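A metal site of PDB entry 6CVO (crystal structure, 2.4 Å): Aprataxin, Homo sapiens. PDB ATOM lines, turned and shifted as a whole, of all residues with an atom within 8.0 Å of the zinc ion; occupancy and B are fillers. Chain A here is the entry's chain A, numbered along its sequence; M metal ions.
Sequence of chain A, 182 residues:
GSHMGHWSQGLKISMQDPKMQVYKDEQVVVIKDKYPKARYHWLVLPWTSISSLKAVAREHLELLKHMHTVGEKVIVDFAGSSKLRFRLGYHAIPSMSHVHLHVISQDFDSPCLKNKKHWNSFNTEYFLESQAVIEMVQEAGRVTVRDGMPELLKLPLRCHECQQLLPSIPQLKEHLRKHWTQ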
ATOM      1  N   ARG A 158      24.334  -8.293  -1.301  1.00  0.00           N
ATOM      2  CA  ARG A 158      25.682  -7.767  -1.191  1.00  0.00           C
ATOM      3  C   ARG A 158      26.010  -7.540   0.272  1.00  0.00           C
ATOM      4  O   ARG A 158      25.184  -6.990   1.016  1.00  0.00           O
ATOM      5  CB  ARG A 158      25.841  -6.462  -1.985  1.00  0.00           C
ATOM      6  CG  ARG A 158      27.279  -5.961  -2.059  1.00  0.00           C
ATOM      7  CD  ARG A 158      27.374  -4.595  -2.725  1.00  0.00           C
ATOM      8  NE  ARG A 158      27.073  -4.655  -4.161  1.00  0.00           N
ATOM      9  CZ  ARG A 158      27.945  -5.035  -5.091  1.00  0.00           C
ATOM     10  NH1 ARG A 158      29.165  -5.419  -4.747  1.00  0.00           N
ATOM     11  NH2 ARG A 158      27.586  -5.047  -6.364  1.00  0.00           N
ATOM     12  N   CYS A 159      27.192  -7.963   0.693  1.00  0.00           N
ATOM     13  CA  CYS A 159      27.611  -7.774   2.066  1.00  0.00           C
ATOM     14  C   CYS A 159      27.851  -6.298   2.356  1.00  0.00           C
ATOM     15  O   CYS A 159      28.484  -5.583   1.581  1.00  0.00           O
ATOM     16  CB  CYS A 159      28.883  -8.565   2.355  1.00  0.00           C
ATOM     17  SG  CYS A 159      29.481  -8.384   4.052  1.00  0.00           S
ATOM     18  N   HIS A 160      27.345  -5.840   3.500  1.00  0.00           N
ATOM     19  CA  HIS A 160      27.483  -4.448   3.891  1.00  0.00           C
ATOM     20  C   HIS A 160      28.856  -4.128   4.490  1.00  0.00           C
ATOM     21  O   HIS A 160      29.182  -2.946   4.628  1.00  0.00           O
ATOM     22  CB  HIS A 160      26.392  -4.060   4.899  1.00  0.00           C
ATOM     23  CG  HIS A 160      26.496  -4.772   6.210  1.00  0.00           C
ATOM     24  ND1 HIS A 160      26.457  -6.145   6.323  1.00  0.00           N
ATOM     25  CD2 HIS A 160      26.602  -4.298   7.471  1.00  0.00           C
ATOM     26  CE1 HIS A 160      26.563  -6.486   7.587  1.00  0.00           C
ATOM     27  NE2 HIS A 160      26.655  -5.392   8.312  1.00  0.00           N
ATOM     28  N   GLU A 161      29.645  -5.134   4.840  1.00  0.00           N
ATOM     29  CA  GLU A 161      30.968  -4.910   5.416  1.00  0.00           C
ATOM     30  C   GLU A 161      32.063  -4.896   4.348  1.00  0.00           C
ATOM     31  O   GLU A 161      32.924  -4.012   4.362  1.00  0.00           O
ATOM     32  CB  GLU A 161      31.269  -5.982   6.474  1.00  0.00           C
ATOM     33  CG  GLU A 161      30.317  -5.965   7.659  1.00  0.00           C
ATOM     34  CD  GLU A 161      30.458  -4.724   8.502  1.00  0.00           C
ATOM     35  OE1 GLU A 161      31.401  -3.941   8.261  1.00  0.00           O
ATOM     36  OE2 GLU A 161      29.617  -4.526   9.406  1.00  0.00           O
ATOM     37  N   CYS A 162      32.040  -5.865   3.433  1.00  0.00           N
ATOM     38  CA  CYS A 162      33.079  -6.000   2.417  1.00  0.00           C
ATOM     39  C   CYS A 162      32.564  -5.838   1.001  1.00  0.00           C
ATOM     40  O   CYS A 162      33.378  -5.844   0.060  1.00  0.00           O
ATOM     41  CB  CYS A 162      33.782  -7.359   2.549  1.00  0.00           C
ATOM     42  SG  CYS A 162      32.786  -8.766   2.014  1.00  0.00           S
ATOM     43  N   GLN A 163      31.249  -5.695   0.802  1.00  0.00           N
ATOM     44  CA  GLN A 163      30.629  -5.433  -0.499  1.00  0.00           C
ATOM     45  C   GLN A 163      30.604  -6.668  -1.398  1.00  0.00           C
ATOM     46  O   GLN A 163      30.267  -6.541  -2.589  1.00  0.00           O
ATOM     47  CB  GLN A 163      31.325  -4.306  -1.258  1.00  0.00           C
ATOM     48  CG  GLN A 163      31.521  -3.034  -0.438  1.00  0.00           C
ATOM     49  CD  GLN A 163      30.206  -2.480   0.078  1.00  0.00           C
ATOM     50  OE1 GLN A 163      29.164  -2.636  -0.555  1.00  0.00           O
ATOM     51  NE2 GLN A 163      30.261  -1.832   1.230  1.00  0.00           N
ATOM     52  N   GLN A 164      30.926  -7.854  -0.886  1.00  0.00           N
ATOM     53  CA  GLN A 164      30.930  -9.049  -1.721  1.00  0.00           C
ATOM     54  C   GLN A 164      29.508  -9.469  -2.065  1.00  0.00           C
ATOM     55  O   GLN A 164      28.604  -9.419  -1.215  1.00  0.00           O
ATOM     56  CB  GLN A 164      31.666 -10.177  -1.014  1.00  0.00           C
ATOM     57  CG  GLN A 164      31.763 -11.462  -1.829  1.00  0.00           C
ATOM     58  CD  GLN A 164      32.655 -12.506  -1.177  1.00  0.00           C
ATOM     59  OE1 GLN A 164      33.607 -12.165  -0.480  1.00  0.00           O
ATOM     60  NE2 GLN A 164      32.356 -13.776  -1.406  1.00  0.00           N
ATOM     61  N   LEU A 165      29.307  -9.894  -3.310  1.00  0.00           N
ATOM     62  CA  LEU A 165      28.015 -10.397  -3.738  1.00  0.00           C
ATOM     63  C   LEU A 165      27.849 -11.854  -3.322  1.00  0.00           C
ATOM     64  O   LEU A 165      28.748 -12.675  -3.530  1.00  0.00           O
ATOM     65  CB  LEU A 165      27.875 -10.276  -5.257  1.00  0.00           C
ATOM     66  CG  LEU A 165      27.779  -8.874  -5.856  1.00  0.00           C
ATOM     67  CD1 LEU A 165      27.905  -8.929  -7.373  1.00  0.00           C
ATOM     68  CD2 LEU A 165      26.467  -8.209  -5.460  1.00  0.00           C
ATOM     69  N   LEU A 166      26.698 -12.178  -2.726  1.00  0.00           N
ATOM     70  CA  LEU A 166      26.397 -13.535  -2.347  1.00  0.00           C
ATOM     71  C   LEU A 166      25.152 -14.016  -3.089  1.00  0.00           C
ATOM     72  O   LEU A 166      24.252 -13.221  -3.392  1.00  0.00           O
ATOM     73  CB  LEU A 166      26.168 -13.671  -0.832  1.00  0.00           C
ATOM     74  CG  LEU A 166      27.372 -13.488   0.091  1.00  0.00           C
ATOM     75  CD1 LEU A 166      28.581 -14.299  -0.371  1.00  0.00           C
ATOM     76  CD2 LEU A 166      27.727 -12.016   0.252  1.00  0.00           C
ATOM     77  N   LEU A 172      24.716 -15.951   2.516  1.00  0.00           N
ATOM     78  CA  LEU A 172      24.990 -14.648   3.112  1.00  0.00           C
ATOM     79  C   LEU A 172      25.157 -14.767   4.618  1.00  0.00           C
ATOM     80  O   LEU A 172      26.108 -14.216   5.197  1.00  0.00           O
ATOM     81  CB  LEU A 172      23.875 -13.666   2.775  1.00  0.00           C
ATOM     82  CG  LEU A 172      23.904 -12.333   3.536  1.00  0.00           C
ATOM     83  CD1 LEU A 172      25.242 -11.631   3.367  1.00  0.00           C
ATOM     84  CD2 LEU A 172      22.768 -11.427   3.079  1.00  0.00           C
ATOM     85  N   HIS A 175      28.416 -16.123   5.324  1.00  0.00           N
ATOM     86  CA  HIS A 175      29.443 -15.125   5.075  1.00  0.00           C
ATOM     87  C   HIS A 175      29.546 -14.134   6.224  1.00  0.00           C
ATOM     88  O   HIS A 175      30.652 -13.745   6.623  1.00  0.00           O
ATOM     89  CB  HIS A 175      29.149 -14.395   3.763  1.00  0.00           C
ATOM     90  CG  HIS A 175      30.058 -13.242   3.492  1.00  0.00           C
ATOM     91  ND1 HIS A 175      31.250 -13.372   2.816  1.00  0.00           N
ATOM     92  CD2 HIS A 175      29.946 -11.937   3.817  1.00  0.00           C
ATOM     93  CE1 HIS A 175      31.833 -12.183   2.726  1.00  0.00           C
ATOM     94  NE2 HIS A 175      31.067 -11.300   3.332  1.00  0.00           N
ATOM     95  N   LEU A 176      28.404 -13.700   6.763  1.00  0.00           N
ATOM     96  CA  LEU A 176      28.406 -12.719   7.842  1.00  0.00           C
ATOM     97  C   LEU A 176      29.170 -13.201   9.071  1.00  0.00           C
ATOM     98  O   LEU A 176      29.612 -12.380   9.869  1.00  0.00           O
ATOM     99  CB  LEU A 176      26.973 -12.344   8.229  1.00  0.00           C
ATOM    100  CG  LEU A 176      26.122 -11.602   7.193  1.00  0.00           C
ATOM    101  CD1 LEU A 176      24.750 -11.305   7.769  1.00  0.00           C
ATOM    102  CD2 LEU A 176      26.791 -10.323   6.717  1.00  0.00           C
ATOM    103  N   ARG A 177      29.313 -14.515   9.246  1.00  0.00           N
ATOM    104  CA  ARG A 177      30.052 -15.021  10.397  1.00  0.00           C
ATOM    105  C   ARG A 177      31.505 -14.584  10.369  1.00  0.00           C
ATOM    106  O   ARG A 177      32.122 -14.440  11.432  1.00  0.00           O
ATOM    107  CB  ARG A 177      29.964 -16.548  10.438  1.00  0.00           C
ATOM    108  CG  ARG A 177      28.544 -17.090  10.592  1.00  0.00           C
ATOM    109  CD  ARG A 177      28.530 -18.604  10.743  1.00  0.00           C
ATOM    110  NE  ARG A 177      28.199 -19.016  12.107  1.00  0.00           N
ATOM    111  CZ  ARG A 177      29.086 -19.297  13.060  1.00  0.00           C
ATOM    112  NH1 ARG A 177      30.389 -19.220  12.821  1.00  0.00           N
ATOM    113  NH2 ARG A 177      28.674 -19.670  14.263  1.00  0.00           N
ATOM    114  N   LYS A 178      32.053 -14.337   9.184  1.00  0.00           N
ATOM    115  CA  LYS A 178      33.440 -13.896   9.087  1.00  0.00           C
ATOM    116  C   LYS A 178      33.630 -12.481   9.614  1.00  0.00           C
ATOM    117  O   LYS A 178      34.768 -12.104   9.939  1.00  0.00           O
ATOM    118  CB  LYS A 178      33.919 -13.980   7.630  1.00  0.00           C
ATOM    119  CG  LYS A 178      33.900 -15.392   7.067  1.00  0.00           C
ATOM    120  CD  LYS A 178      34.468 -15.449   5.659  1.00  0.00           C
ATOM    121  CE  LYS A 178      33.581 -14.705   4.665  1.00  0.00           C
ATOM    122  NZ  LYS A 178      34.060 -14.876   3.266  1.00  0.00           N
ATOM    123  N   HIS A 179      32.563 -11.690   9.701  1.00  0.00           N
ATOM    124  CA  HIS A 179      32.654 -10.341  10.243  1.00  0.00           C
ATOM    125  C   HIS A 179      32.104 -10.307  11.663  1.00  0.00           C
ATOM    126  O   HIS A 179      32.483  -9.451  12.474  1.00  0.00           O
ATOM    127  CB  HIS A 179      31.884  -9.357   9.356  1.00  0.00           C
ATOM    128  CG  HIS A 179      32.258  -9.421   7.914  1.00  0.00           C
ATOM    129  ND1 HIS A 179      33.560  -9.278   7.471  1.00  0.00           N
ATOM    130  CD2 HIS A 179      31.504  -9.604   6.793  1.00  0.00           C
ATOM    131  CE1 HIS A 179      33.585  -9.375   6.156  1.00  0.00           C
ATOM    132  NE2 HIS A 179      32.355  -9.579   5.727  1.00  0.00           N
HETATM  133 ZN    ZN M   1      31.667  -9.443   3.765  1.00  0.00          ZN
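SG of Cys 159 lies close to N of Glu 161.
The side-chain amino group (NZ) of Lys 178 sits at hydrogen-bond distance from a ring nitrogen (ND1) of His 175, at 3.2 Å.
The backbone NH of Cys 159 sits at hydrogen-bond distance from the backbone carbonyl oxygen of Gln 164, at 2.8 Å.
SG of Cys 162 sits close to N of Gln 164 (3.6 Å).
Of the 15 residues printed, 4 come within 4 Å of the zinc ion.
The zinc ion is bound by a ring nitrogen (NE2) of His 175.
The zinc ion is bound by a ring nitrogen (NE2) of His 179, at 2.1 Å.
SG of Cys 162 is bound to the zinc ion (2.2 Å).
The zinc ion is bound by SG of Cys 159, at 2.4 Å.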
